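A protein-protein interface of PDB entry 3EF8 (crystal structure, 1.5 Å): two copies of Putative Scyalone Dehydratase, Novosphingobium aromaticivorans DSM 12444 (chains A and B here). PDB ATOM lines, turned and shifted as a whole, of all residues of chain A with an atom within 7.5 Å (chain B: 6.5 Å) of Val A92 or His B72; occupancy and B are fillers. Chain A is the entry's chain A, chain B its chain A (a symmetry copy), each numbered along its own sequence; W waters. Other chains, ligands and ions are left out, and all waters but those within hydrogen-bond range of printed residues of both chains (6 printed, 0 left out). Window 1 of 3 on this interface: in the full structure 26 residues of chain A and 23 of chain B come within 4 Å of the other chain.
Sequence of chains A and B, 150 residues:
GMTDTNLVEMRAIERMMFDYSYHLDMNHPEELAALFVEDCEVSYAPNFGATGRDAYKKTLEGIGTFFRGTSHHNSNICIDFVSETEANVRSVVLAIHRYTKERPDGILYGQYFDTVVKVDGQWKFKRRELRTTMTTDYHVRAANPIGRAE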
ATOM      1  N   MET A  17       2.012  -2.756  28.788  1.00  0.00           N
ATOM      2  CA  MET A  17       0.716  -2.393  29.354  1.00  0.00           C
ATOM      3  C   MET A  17       0.553  -2.990  30.760  1.00  0.00           C
ATOM      4  O   MET A  17      -0.033  -2.355  31.646  1.00  0.00           O
ATOM      5  CB  MET A  17      -0.424  -2.819  28.449  1.00  0.00           C
ATOM      6  CG  MET A  17      -0.359  -2.112  27.055  1.00  0.00           C
ATOM      7  SD  MET A  17      -1.626  -2.785  25.818  1.00  0.00           S
ATOM      8  CE  MET A  17      -3.323  -2.218  26.603  1.00  0.00           C
ATOM      9  N   HIS A  73      -6.885  -4.978  36.150  1.00  0.00           N
ATOM     10  CA  HIS A  73      -6.999  -6.224  35.422  1.00  0.00           C
ATOM     11  C   HIS A  73      -7.266  -5.849  33.967  1.00  0.00           C
ATOM     12  O   HIS A  73      -8.336  -5.354  33.629  1.00  0.00           O
ATOM     13  CB  HIS A  73      -8.190  -7.035  35.982  1.00  0.00           C
ATOM     14  CG  HIS A  73      -8.110  -7.236  37.468  1.00  0.00           C
ATOM     15  ND1 HIS A  73      -7.775  -8.457  38.025  1.00  0.00           N
ATOM     16  CD2 HIS A  73      -8.235  -6.361  38.496  1.00  0.00           C
ATOM     17  CE1 HIS A  73      -7.695  -8.303  39.349  1.00  0.00           C
ATOM     18  NE2 HIS A  73      -7.947  -7.045  39.652  1.00  0.00           N
ATOM     19  N   ASN A  74      -6.307  -6.125  33.092  1.00  0.00           N
ATOM     20  CA  ASN A  74      -6.343  -5.689  31.705  1.00  0.00           C
ATOM     21  C   ASN A  74      -6.472  -6.883  30.825  1.00  0.00           C
ATOM     22  O   ASN A  74      -5.660  -7.819  30.951  1.00  0.00           O
ATOM     23  CB  ASN A  74      -5.046  -4.977  31.368  1.00  0.00           C
ATOM     24  CG  ASN A  74      -4.803  -3.788  32.262  1.00  0.00           C
ATOM     25  OD1 ASN A  74      -4.204  -3.884  33.348  1.00  0.00           O
ATOM     26  ND2 ASN A  74      -5.257  -2.628  31.799  1.00  0.00           N
ATOM     27  N   SER A  75      -7.471  -6.875  29.951  1.00  0.00           N
ATOM     28  CA  SER A  75      -7.783  -8.037  29.147  1.00  0.00           C
ATOM     29  C   SER A  75      -8.291  -7.591  27.779  1.00  0.00           C
ATOM     30  O   SER A  75      -8.437  -6.392  27.496  1.00  0.00           O
ATOM     31  CB  SER A  75      -8.866  -8.892  29.823  1.00  0.00           C
ATOM     32  OG  SER A  75     -10.101  -8.228  29.906  1.00  0.00           O
ATOM     33  N   ASN A  76      -8.598  -8.543  26.933  1.00  0.00           N
ATOM     34  CA  ASN A  76      -9.250  -8.262  25.667  1.00  0.00           C
ATOM     35  C   ASN A  76      -8.410  -7.322  24.811  1.00  0.00           C
ATOM     36  O   ASN A  76      -8.985  -6.450  24.118  1.00  0.00           O
ATOM     37  CB  ASN A  76     -10.665  -7.676  25.875  1.00  0.00           C
ATOM     38  CG  ASN A  76     -11.625  -8.628  26.559  1.00  0.00           C
ATOM     39  OD1 ASN A  76     -11.371  -9.103  27.647  1.00  0.00           O
ATOM     40  ND2 ASN A  76     -12.755  -8.871  25.928  1.00  0.00           N
ATOM     41  N   ILE A  77      -7.103  -7.533  24.785  1.00  0.00           N
ATOM     42  CA  ILE A  77      -6.161  -6.644  24.103  1.00  0.00           C
ATOM     43  C   ILE A  77      -6.091  -6.958  22.610  1.00  0.00           C
ATOM     44  O   ILE A  77      -5.795  -8.068  22.243  1.00  0.00           O
ATOM     45  CB  ILE A  77      -4.790  -6.703  24.753  1.00  0.00           C
ATOM     46  CG1 ILE A  77      -4.857  -6.179  26.224  1.00  0.00           C
ATOM     47  CG2 ILE A  77      -3.766  -5.858  23.960  1.00  0.00           C
ATOM     48  CD1 ILE A  77      -3.616  -6.439  27.059  1.00  0.00           C
ATOM     49  N   CYS A  78      -6.427  -5.960  21.793  1.00  0.00           N
ATOM     50  CA  CYS A  78      -6.517  -6.026  20.316  1.00  0.00           C
ATOM     51  C   CYS A  78      -5.521  -5.030  19.760  1.00  0.00           C
ATOM     52  O   CYS A  78      -5.579  -3.852  20.067  1.00  0.00           O
ATOM     53  CB  CYS A  78      -7.917  -5.640  19.920  1.00  0.00           C
ATOM     54  SG  CYS A  78      -9.171  -6.764  20.565  1.00  0.00           S
ATOM     55  N   ARG A  90      -6.818  -1.558  21.350  1.00  0.00           N
ATOM     56  CA  ARG A  90      -8.090  -1.470  22.056  1.00  0.00           C
ATOM     57  C   ARG A  90      -8.069  -2.539  23.112  1.00  0.00           C
ATOM     58  O   ARG A  90      -7.647  -3.677  22.865  1.00  0.00           O
ATOM     59  CB  ARG A  90      -9.287  -1.721  21.144  1.00  0.00           C
ATOM     60  CG  ARG A  90     -10.637  -1.562  21.832  1.00  0.00           C
ATOM     61  CD  ARG A  90     -11.777  -2.015  20.934  1.00  0.00           C
ATOM     62  NE  ARG A  90     -11.780  -3.457  20.797  1.00  0.00           N
ATOM     63  CZ  ARG A  90     -12.135  -4.100  19.707  1.00  0.00           C
ATOM     64  NH1 ARG A  90     -12.462  -3.444  18.604  1.00  0.00           N
ATOM     65  NH2 ARG A  90     -12.156  -5.406  19.732  1.00  0.00           N
ATOM     66  N   SER A  91      -8.465  -2.195  24.334  1.00  0.00           N
ATOM     67  CA  SER A  91      -8.482  -3.181  25.412  1.00  0.00           C
ATOM     68  C   SER A  91      -9.541  -2.852  26.444  1.00  0.00           C
ATOM     69  O   SER A  91     -10.174  -1.798  26.401  1.00  0.00           O
ATOM     70  CB  SER A  91      -7.145  -3.277  26.109  1.00  0.00           C
ATOM     71  OG  SER A  91      -6.800  -2.042  26.747  1.00  0.00           O
ATOM     72  N   VAL A  92      -9.792  -3.825  27.292  1.00  0.00           N
ATOM     73  CA  VAL A  92     -10.757  -3.714  28.387  1.00  0.00           C
ATOM     74  C   VAL A  92     -10.030  -3.668  29.711  1.00  0.00           C
ATOM     75  O   VAL A  92      -8.980  -4.294  29.890  1.00  0.00           O
ATOM     76  CB  VAL A  92     -11.765  -4.884  28.357  1.00  0.00           C
ATOM     77  CG1 VAL A  92     -12.675  -4.894  29.596  1.00  0.00           C
ATOM     78  CG2 VAL A  92     -12.609  -4.820  27.095  1.00  0.00           C
ATOM     79  N   VAL A  93     -10.550  -2.844  30.626  1.00  0.00           N
ATOM     80  CA  VAL A  93     -10.000  -2.719  31.970  1.00  0.00           C
ATOM     81  C   VAL A  93     -11.069  -2.850  33.024  1.00  0.00           C
ATOM     82  O   VAL A  93     -12.178  -2.359  32.874  1.00  0.00           O
ATOM     83  CB  VAL A  93      -9.167  -1.400  32.142  1.00  0.00           C
ATOM     84  CG1 VAL A  93     -10.037  -0.168  31.991  1.00  0.00           C
ATOM     85  CG2 VAL A  93      -8.456  -1.395  33.465  1.00  0.00           C
ATOM     86  N   LEU A  94     -10.716  -3.578  34.076  1.00  0.00           N
ATOM     87  CA  LEU A  94     -11.443  -3.632  35.336  1.00  0.00           C
ATOM     88  C   LEU A  94     -10.479  -3.041  36.380  1.00  0.00           C
ATOM     89  O   LEU A  94      -9.389  -3.550  36.592  1.00  0.00           O
ATOM     90  CB  LEU A  94     -11.814  -5.050  35.721  1.00  0.00           C
ATOM     91  CG  LEU A  94     -12.514  -5.241  37.052  1.00  0.00           C
ATOM     92  CD1 LEU A  94     -13.902  -4.609  37.032  1.00  0.00           C
ATOM     93  CD2 LEU A  94     -12.598  -6.765  37.331  1.00  0.00           C
ATOM     94  N   TYR A 109     -15.226   0.058  35.017  1.00  0.00           N
ATOM     95  CA  TYR A 109     -15.298  -0.863  33.872  1.00  0.00           C
ATOM     96  C   TYR A 109     -15.038  -0.028  32.643  1.00  0.00           C
ATOM     97  O   TYR A 109     -15.799   0.889  32.360  1.00  0.00           O
ATOM     98  CB  TYR A 109     -16.644  -1.523  33.761  1.00  0.00           C
ATOM     99  CG  TYR A 109     -17.120  -2.217  34.999  1.00  0.00           C
ATOM    100  CD1 TYR A 109     -16.813  -3.544  35.267  1.00  0.00           C
ATOM    101  CD2 TYR A 109     -17.888  -1.510  35.920  1.00  0.00           C
ATOM    102  CE1 TYR A 109     -17.280  -4.178  36.416  1.00  0.00           C
ATOM    103  CE2 TYR A 109     -18.392  -2.139  37.039  1.00  0.00           C
ATOM    104  CZ  TYR A 109     -18.071  -3.465  37.290  1.00  0.00           C
ATOM    105  OH  TYR A 109     -18.574  -4.092  38.417  1.00  0.00           O
ATOM    106  N   GLY A 110     -13.938  -0.275  31.940  1.00  0.00           N
ATOM    107  CA  GLY A 110     -13.558   0.644  30.897  1.00  0.00           C
ATOM    108  C   GLY A 110     -12.969  -0.013  29.665  1.00  0.00           C
ATOM    109  O   GLY A 110     -12.768  -1.241  29.621  1.00  0.00           O
ATOM    110  N   GLN A 111     -12.726   0.829  28.691  1.00  0.00           N
ATOM    111  CA  GLN A 111     -12.020   0.486  27.459  1.00  0.00           C
ATOM    112  C   GLN A 111     -10.898   1.468  27.269  1.00  0.00           C
ATOM    113  O   GLN A 111     -11.115   2.682  27.439  1.00  0.00           O
ATOM    114  CB  GLN A 111     -12.964   0.585  26.257  1.00  0.00           C
ATOM    115  CG  GLN A 111     -14.240  -0.187  26.402  1.00  0.00           C
ATOM    116  CD  GLN A 111     -15.221   0.087  25.244  1.00  0.00           C
ATOM    117  OE1 GLN A 111     -15.027   1.062  24.493  1.00  0.00           O
ATOM    118  NE2 GLN A 111     -16.266  -0.718  25.129  1.00  0.00           N
ATOM    119  N   TYR A 112      -9.735   1.007  26.890  1.00  0.00           N
ATOM    120  CA  TYR A 112      -8.668   1.881  26.485  1.00  0.00           C
ATOM    121  C   TYR A 112      -8.454   1.842  25.001  1.00  0.00           C
ATOM    122  O   TYR A 112      -8.300   0.775  24.440  1.00  0.00           O
ATOM    123  CB  TYR A 112      -7.352   1.510  27.175  1.00  0.00           C
ATOM    124  CG  TYR A 112      -7.107   2.155  28.494  1.00  0.00           C
ATOM    125  CD1 TYR A 112      -6.878   3.508  28.550  1.00  0.00           C
ATOM    126  CD2 TYR A 112      -7.069   1.430  29.639  1.00  0.00           C
ATOM    127  CE1 TYR A 112      -6.613   4.158  29.706  1.00  0.00           C
ATOM    128  CE2 TYR A 112      -6.782   2.098  30.884  1.00  0.00           C
ATOM    129  CZ  TYR A 112      -6.555   3.441  30.862  1.00  0.00           C
ATOM    130  OH  TYR A 112      -6.307   4.161  32.050  1.00  0.00           O
ATOM    131  N   THR A 133     -17.199   2.460  30.357  1.00  0.00           N
ATOM    132  CA  THR A 133     -18.360   1.633  30.111  1.00  0.00           C
ATOM    133  C   THR A 133     -19.397   1.810  31.177  1.00  0.00           C
ATOM    134  O   THR A 133     -20.583   1.947  30.897  1.00  0.00           O
ATOM    135  CB  THR A 133     -17.917   0.147  30.038  1.00  0.00           C
ATOM    136  OG1 THR A 133     -16.836   0.072  29.114  1.00  0.00           O
ATOM    137  CG2 THR A 133     -19.057  -0.795  29.630  1.00  0.00           C
ATOM    138  N   MET A 134     -18.923   1.838  32.416  1.00  0.00           N
ATOM    139  CA  MET A 134     -19.738   2.144  33.567  1.00  0.00           C
ATOM    140  C   MET A 134     -18.865   2.122  34.774  1.00  0.00           C
ATOM    141  O   MET A 134     -17.710   1.702  34.725  1.00  0.00           O
ATOM    142  CB  MET A 134     -20.883   1.174  33.711  1.00  0.00           C
ATOM    143  CG  MET A 134     -20.482  -0.229  33.655  1.00  0.00           C
ATOM    144  SD  MET A 134     -22.009  -1.239  32.987  1.00  0.00           S
ATOM    145  CE  MET A 134     -21.661  -2.725  34.037  1.00  0.00           C
ATOM    146  N   TYR B  20     -15.992  -9.798  19.395  1.00  0.00           N
ATOM    147  CA  TYR B  20     -17.336 -10.205  19.803  1.00  0.00           C
ATOM    148  C   TYR B  20     -17.811  -9.510  21.082  1.00  0.00           C
ATOM    149  O   TYR B  20     -18.869  -8.891  21.138  1.00  0.00           O
ATOM    150  CB  TYR B  20     -17.452 -11.749  19.958  1.00  0.00           C
ATOM    151  CG  TYR B  20     -18.765 -12.237  20.520  1.00  0.00           C
ATOM    152  CD1 TYR B  20     -18.974 -12.257  21.872  1.00  0.00           C
ATOM    153  CD2 TYR B  20     -19.790 -12.661  19.697  1.00  0.00           C
ATOM    154  CE1 TYR B  20     -20.185 -12.689  22.443  1.00  0.00           C
ATOM    155  CE2 TYR B  20     -21.006 -13.096  20.266  1.00  0.00           C
ATOM    156  CZ  TYR B  20     -21.166 -13.098  21.627  1.00  0.00           C
ATOM    157  OH  TYR B  20     -22.362 -13.494  22.233  1.00  0.00           O
ATOM    158  N   SER B  21     -16.963  -9.544  22.103  1.00  0.00           N
ATOM    159  CA  SER B  21     -17.302  -8.951  23.406  1.00  0.00           C
ATOM    160  C   SER B  21     -17.440  -7.443  23.291  1.00  0.00           C
ATOM    161  O   SER B  21     -18.313  -6.848  23.931  1.00  0.00           O
ATOM    162  CB  SER B  21     -16.269  -9.311  24.433  1.00  0.00           C
ATOM    163  OG  SER B  21     -16.487 -10.633  24.824  1.00  0.00           O
ATOM    164  N   TYR B  22     -16.600  -6.853  22.459  1.00  0.00           N
ATOM    165  CA  TYR B  22     -16.681  -5.394  22.188  1.00  0.00           C
ATOM    166  C   TYR B  22     -18.011  -5.024  21.546  1.00  0.00           C
ATOM    167  O   TYR B  22     -18.743  -4.151  22.013  1.00  0.00           O
ATOM    168  CB  TYR B  22     -15.529  -4.907  21.319  1.00  0.00           C
ATOM    169  CG  TYR B  22     -15.582  -3.409  21.008  1.00  0.00           C
ATOM    170  CD1 TYR B  22     -15.331  -2.465  21.992  1.00  0.00           C
ATOM    171  CD2 TYR B  22     -15.883  -2.957  19.728  1.00  0.00           C
ATOM    172  CE1 TYR B  22     -15.415  -1.129  21.724  1.00  0.00           C
ATOM    173  CE2 TYR B  22     -15.993  -1.629  19.457  1.00  0.00           C
ATOM    174  CZ  TYR B  22     -15.718  -0.710  20.433  1.00  0.00           C
ATOM    175  OH  TYR B  22     -15.783   0.661  20.120  1.00  0.00           O
ATOM    176  N   LEU B  24     -20.704  -6.623  21.551  1.00  0.00           N
ATOM    177  CA  LEU B  24     -21.771  -6.945  22.472  1.00  0.00           C
ATOM    178  C   LEU B  24     -21.952  -5.772  23.465  1.00  0.00           C
ATOM    179  O   LEU B  24     -23.063  -5.295  23.676  1.00  0.00           O
ATOM    180  CB  LEU B  24     -21.433  -8.253  23.222  1.00  0.00           C
ATOM    181  CG  LEU B  24     -22.450  -8.701  24.249  1.00  0.00           C
ATOM    182  CD1 LEU B  24     -23.905  -8.808  23.671  1.00  0.00           C
ATOM    183  CD2 LEU B  24     -22.011 -10.053  24.869  1.00  0.00           C
ATOM    184  N   ASP B  25     -20.837  -5.308  24.053  1.00  0.00           N
ATOM    185  CA  ASP B  25     -20.901  -4.197  24.992  1.00  0.00           C
ATOM    186  C   ASP B  25     -21.340  -2.911  24.286  1.00  0.00           C
ATOM    187  O   ASP B  25     -21.932  -2.006  24.901  1.00  0.00           O
ATOM    188  CB  ASP B  25     -19.572  -3.991  25.663  1.00  0.00           C
ATOM    189  CG  ASP B  25     -19.227  -5.088  26.693  1.00  0.00           C
ATOM    190  OD1 ASP B  25     -20.127  -5.852  27.095  1.00  0.00           O
ATOM    191  OD2 ASP B  25     -18.016  -5.226  27.027  1.00  0.00           O
ATOM    192  N   THR B  70     -23.228  -3.169  29.488  1.00  0.00           N
ATOM    193  CA  THR B  70     -22.576  -4.419  29.895  1.00  0.00           C
ATOM    194  C   THR B  70     -21.067  -4.250  29.740  1.00  0.00           C
ATOM    195  O   THR B  70     -20.574  -3.430  28.962  1.00  0.00           O
ATOM    196  CB  THR B  70     -23.045  -5.650  29.071  1.00  0.00           C
ATOM    197  OG1 THR B  70     -22.743  -5.480  27.700  1.00  0.00           O
ATOM    198  CG2 THR B  70     -24.532  -5.901  29.135  1.00  0.00           C
ATOM    199  N   SER B  71     -20.329  -5.057  30.500  1.00  0.00           N
ATOM    200  CA  SER B  71     -18.898  -5.120  30.370  1.00  0.00           C
ATOM    201  C   SER B  71     -18.452  -6.578  30.425  1.00  0.00           C
ATOM    202  O   SER B  71     -18.747  -7.268  31.373  1.00  0.00           O
ATOM    203  CB  SER B  71     -18.248  -4.332  31.499  1.00  0.00           C
ATOM    204  OG  SER B  71     -16.865  -4.143  31.282  1.00  0.00           O
ATOM    205  N   HIS B  72     -17.772  -7.014  29.363  1.00  0.00           N
ATOM    206  CA  HIS B  72     -17.293  -8.379  29.257  1.00  0.00           C
ATOM    207  C   HIS B  72     -15.769  -8.404  29.262  1.00  0.00           C
ATOM    208  O   HIS B  72     -15.095  -7.724  28.525  1.00  0.00           O
ATOM    209  CB  HIS B  72     -17.797  -9.017  27.973  1.00  0.00           C
ATOM    210  CG  HIS B  72     -19.239  -9.343  27.989  1.00  0.00           C
ATOM    211  ND1 HIS B  72     -20.227  -8.379  27.890  1.00  0.00           N
ATOM    212  CD2 HIS B  72     -19.881 -10.521  28.167  1.00  0.00           C
ATOM    213  CE1 HIS B  72     -21.412  -8.956  28.007  1.00  0.00           C
ATOM    214  NE2 HIS B  72     -21.238 -10.262  28.155  1.00  0.00           N
ATOM    215  N   HIS B  73     -15.272  -9.247  30.153  1.00  0.00           N
ATOM    216  CA  HIS B  73     -13.857  -9.418  30.406  1.00  0.00           C
ATOM    217  C   HIS B  73     -13.553 -10.894  30.168  1.00  0.00           C
ATOM    218  O   HIS B  73     -13.970 -11.756  30.934  1.00  0.00           O
ATOM    219  CB  HIS B  73     -13.555  -9.050  31.876  1.00  0.00           C
ATOM    220  CG  HIS B  73     -14.050  -7.682  32.249  1.00  0.00           C
ATOM    221  ND1 HIS B  73     -13.190  -6.612  32.418  1.00  0.00           N
ATOM    222  CD2 HIS B  73     -15.307  -7.197  32.397  1.00  0.00           C
ATOM    223  CE1 HIS B  73     -13.923  -5.521  32.651  1.00  0.00           C
ATOM    224  NE2 HIS B  73     -15.201  -5.846  32.622  1.00  0.00           N
ATOM    225  N   ASN B  74     -12.786 -11.186  29.125  1.00  0.00           N
ATOM    226  CA  ASN B  74     -12.536 -12.546  28.674  1.00  0.00           C
ATOM    227  C   ASN B  74     -11.099 -12.872  28.886  1.00  0.00           C
ATOM    228  O   ASN B  74     -10.231 -12.109  28.424  1.00  0.00           O
ATOM    229  CB  ASN B  74     -12.842 -12.648  27.191  1.00  0.00           C
ATOM    230  CG  ASN B  74     -14.266 -12.269  26.879  1.00  0.00           C
ATOM    231  OD1 ASN B  74     -14.604 -11.097  26.636  1.00  0.00           O
ATOM    232  ND2 ASN B  74     -15.131 -13.277  26.860  1.00  0.00           N
ATOM    233  N   VAL B  93     -15.080 -16.076  31.509  1.00  0.00           N
ATOM    234  CA  VAL B  93     -15.737 -14.788  31.320  1.00  0.00           C
ATOM    235  C   VAL B  93     -16.243 -14.224  32.622  1.00  0.00           C
ATOM    236  O   VAL B  93     -16.747 -14.939  33.476  1.00  0.00           O
ATOM    237  CB  VAL B  93     -16.868 -14.861  30.235  1.00  0.00           C
ATOM    238  CG1 VAL B  93     -17.994 -15.782  30.664  1.00  0.00           C
ATOM    239  CG2 VAL B  93     -17.390 -13.487  29.923  1.00  0.00           C
ATOM    240  N   LEU B  94     -16.041 -12.922  32.771  1.00  0.00           N
ATOM    241  CA  LEU B  94     -16.664 -12.090  33.791  1.00  0.00           C
ATOM    242  C   LEU B  94     -17.541 -11.091  33.012  1.00  0.00           C
ATOM    243  O   LEU B  94     -17.051 -10.324  32.198  1.00  0.00           O
ATOM    244  CB  LEU B  94     -15.644 -11.340  34.621  1.00  0.00           C
ATOM    245  CG  LEU B  94     -16.176 -10.387  35.672  1.00  0.00           C
ATOM    246  CD1 LEU B  94     -16.900 -11.146  36.779  1.00  0.00           C
ATOM    247  CD2 LEU B  94     -14.975  -9.584  36.238  1.00  0.00           C
ATOM    248  N   ALA B  95     -18.853 -11.108  33.251  1.00  0.00           N
ATOM    249  CA  ALA B  95     -19.764 -10.262  32.513  1.00  0.00           C
ATOM    250  C   ALA B  95     -20.662  -9.519  33.489  1.00  0.00           C
ATOM    251  O   ALA B  95     -21.341 -10.141  34.283  1.00  0.00           O
ATOM    252  CB  ALA B  95     -20.603 -11.088  31.512  1.00  0.00           C
ATOM    253  N   ILE B  96     -20.574  -8.183  33.437  1.00  0.00           N
ATOM    254  CA  ILE B  96     -21.346  -7.326  34.361  1.00  0.00           C
ATOM    255  C   ILE B  96     -22.437  -6.646  33.552  1.00  0.00           C
ATOM    256  O   ILE B  96     -22.212  -6.129  32.508  1.00  0.00           O
ATOM    257  CB  ILE B  96     -20.460  -6.306  35.044  1.00  0.00           C
ATOM    258  CG1 ILE B  96     -19.285  -6.980  35.799  1.00  0.00           C
ATOM    259  CG2 ILE B  96     -21.291  -5.472  36.059  1.00  0.00           C
ATOM    260  CD1 ILE B  96     -18.017  -7.168  34.910  1.00  0.00           C
ATOM    261  N   HIS B  97     -23.637  -6.685  34.109  1.00  0.00           N
ATOM    262  CA  HIS B  97     -24.821  -6.138  33.458  1.00  0.00           C
ATOM    263  C   HIS B  97     -25.516  -5.070  34.297  1.00  0.00           C
ATOM    264  O   HIS B  97     -25.903  -5.349  35.439  1.00  0.00           O
ATOM    265  CB  HIS B  97     -25.820  -7.281  33.231  1.00  0.00           C
ATOM    266  CG  HIS B  97     -25.263  -8.441  32.480  1.00  0.00           C
ATOM    267  ND1 HIS B  97     -24.421  -9.348  33.088  1.00  0.00           N
ATOM    268  CD2 HIS B  97     -25.433  -8.863  31.210  1.00  0.00           C
ATOM    269  CE1 HIS B  97     -24.060 -10.256  32.198  1.00  0.00           C
ATOM    270  NE2 HIS B  97     -24.676 -10.001  31.063  1.00  0.00           N
ATOM    271  N   LEU B 108     -22.192 -12.349  35.944  1.00  0.00           N
ATOM    272  CA  LEU B 108     -22.018 -13.707  35.470  1.00  0.00           C
ATOM    273  C   LEU B 108     -20.529 -14.049  35.535  1.00  0.00           C
ATOM    274  O   LEU B 108     -19.689 -13.321  35.021  1.00  0.00           O
ATOM    275  CB  LEU B 108     -22.511 -13.872  34.025  1.00  0.00           C
ATOM    276  CG  LEU B 108     -21.972 -15.124  33.282  1.00  0.00           C
ATOM    277  CD1 LEU B 108     -22.725 -16.189  33.918  1.00  0.00           C
ATOM    278  CD2 LEU B 108     -22.272 -15.031  31.767  1.00  0.00           C
ATOM    279  N   TYR B 112     -16.645 -20.461  28.721  1.00  0.00           N
ATOM    280  CA  TYR B 112     -17.091 -20.767  27.389  1.00  0.00           C
ATOM    281  C   TYR B 112     -16.347 -21.934  26.811  1.00  0.00           C
ATOM    282  O   TYR B 112     -15.132 -21.937  26.811  1.00  0.00           O
ATOM    283  CB  TYR B 112     -16.913 -19.566  26.454  1.00  0.00           C
ATOM    284  CG  TYR B 112     -18.055 -18.613  26.399  1.00  0.00           C
ATOM    285  CD1 TYR B 112     -19.240 -19.013  25.834  1.00  0.00           C
ATOM    286  CD2 TYR B 112     -17.938 -17.344  26.863  1.00  0.00           C
ATOM    287  CE1 TYR B 112     -20.309 -18.192  25.716  1.00  0.00           C
ATOM    288  CE2 TYR B 112     -19.060 -16.447  26.743  1.00  0.00           C
ATOM    289  CZ  TYR B 112     -20.202 -16.910  26.162  1.00  0.00           C
ATOM    290  OH  TYR B 112     -21.349 -16.096  26.049  1.00  0.00           O
HETATM  291  O   HOH W   1     -15.527  -2.344  29.537  1.00  0.00           O
HETATM  292  O   HOH W   2     -15.779   2.389  22.208  1.00  0.00           O
HETATM  293  O   HOH W   3     -10.429  -6.694  32.183  1.00  0.00           O
HETATM  294  O   HOH W   4     -16.331  -2.983  26.900  1.00  0.00           O
HETATM  295  O   HOH W   5     -13.492  -6.853  23.962  1.00  0.00           O
HETATM  296  O   HOH W   6      -7.782 -11.327  27.682  1.00  0.00           O
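Among the printed residues, pairs that only touch across the chains: Thr A133 with Thr B70 (3.1 Å), Val A92 with His B73 (3.3 Å), Tyr A109 with Ile B96 (3.4 Å), Met A134 with Ile B96 (3.4 Å), Gln A111 with Tyr B22 (3.5 Å), Tyr A109 with Ser B71 (3.6 Å), Val A93 with His B73 (3.6 Å), Arg A90 with Tyr B22 (3.6 Å), Asn A76 with His B72 (3.7 Å), Asn A76 with His B73 (3.7 Å), Leu A94 with His B73 (3.8 Å), Ser A75 with Asn B74 (3.8 Å), Asn A76 with Ser B21 (3.8 Å), Leu A94 with Leu B94 (3.8 Å), Tyr A109 with His B73 (3.9 Å), Val A92 with His B72 (3.9 Å) and Ser A75 with His B73 (3.97 Å).
The backbone carbonyl oxygen (O) of Val A93 lies within hydrogen-bond range of the backbone NH (N) of Gly A110 (2.9 Å). O of Met A134 sits at hydrogen-bond distance from N of Tyr A109, 3.0 Å away. O of Asn A76 lies within hydrogen-bond range of SG of Cys A78 (3.6 Å). The side-chain amide oxygen of Asn B74 lies within hydrogen-bond range of the side-chain hydroxyl of Ser B21, 2.7 Å away. The side-chain hydroxyl (OG) of Ser B71 sits at hydrogen-bond distance from a ring nitrogen (NE2) of His B73. N of Cys A78 lies within hydrogen-bond range of O of Arg A90, at 2.8 Å.
Val A93 touches His B73, but with the chains exchanged His A73 does not touch Val B93 (11.3 Å). Leu A94 touches His B73, but with the chains exchanged His A73 does not touch Leu B94 (7.3 Å). Leu A94 touches its own counterpart, Leu B94. Of the 18 pairs that touch across the chains among the printed residues, 1 has its exchanged pair printed and touching as well.
Water W6 lies within hydrogen-bond range of the backbone carbonyl oxygen of Asn B74 (2.7 Å) and the backbone NH of Asn A76 (3.0 Å). Water W2 lies within hydrogen-bond range of OH of Tyr B22 (2.7 Å) and OE1 of Gln A111 (2.7 Å). Water W3 lies within hydrogen-bond range of OG of Ser A75 (2.8 Å), ND1 of His B73 (2.8 Å) and O of His A73 (2.9 Å). Water W1 lies within hydrogen-bond range of the side-chain hydroxyl of Thr A133 (2.8 Å), the side-chain hydroxyl of Ser B71 (2.8 Å) and the backbone carbonyl oxygen of Gly A110 (3.0 Å). Water W4 bridges OD2 of Asp B25 and NE2 of Gln A111. Water W5 lies within hydrogen-bond range of ND2 of Asn A76 (2.9 Å) and N of Tyr B22 (3.5 Å).
Of the 17 printed residues of chain B, 9 touch a printed residue of chain A. Printed residues of chain B that touch a printed residue of chain A: Ser B21, Tyr B22, Thr B70, Ser B71, His B72, His B73, Asn B74, Leu B94 and Ile B96. Hydrophobic or aromatic side chains of chain B that line the printed part of chain A: Tyr B22, His B73, Leu B94 and Ile B96. Of the 18 printed residues of chain A, 10 touch a printed residue of chain B. Hydrophobic or aromatic side chains of chain A within 4 Å of the printed part of chain B: Val A92, Leu A94, Tyr A109 and Met A134. Among the printed residues, no Asp or Glu carboxylate lies within 4 Å of a Lys or Arg side-chain nitrogen of the other chain.
Of the printed residues of chain B, Val A92 touches His B72 and His B73. Of the printed residues of chain B, Val A93 touches His B73 (3.6 Å). Of the printed residues of chain B, Gln A111 touches Tyr B22. Tyr A112 touches none of the printed residues of chain B. Printed residues of chain B within 4 Å of Met A134: Ile B96. Of the printed residues of chain A, Ser B71 touches Tyr A109 (3.6 Å). His B72 touches two residues of chain A. Leu B108 touches none of the printed residues of chain A. The nearest residue of chain A that does not touch His B72 is Ser A75 (5.2 Å).
The side-chain amide oxygen (OD1) of Asn A76 lies within hydrogen-bond range of the backbone NH (N) of Asn B74, 2.9 Å away.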
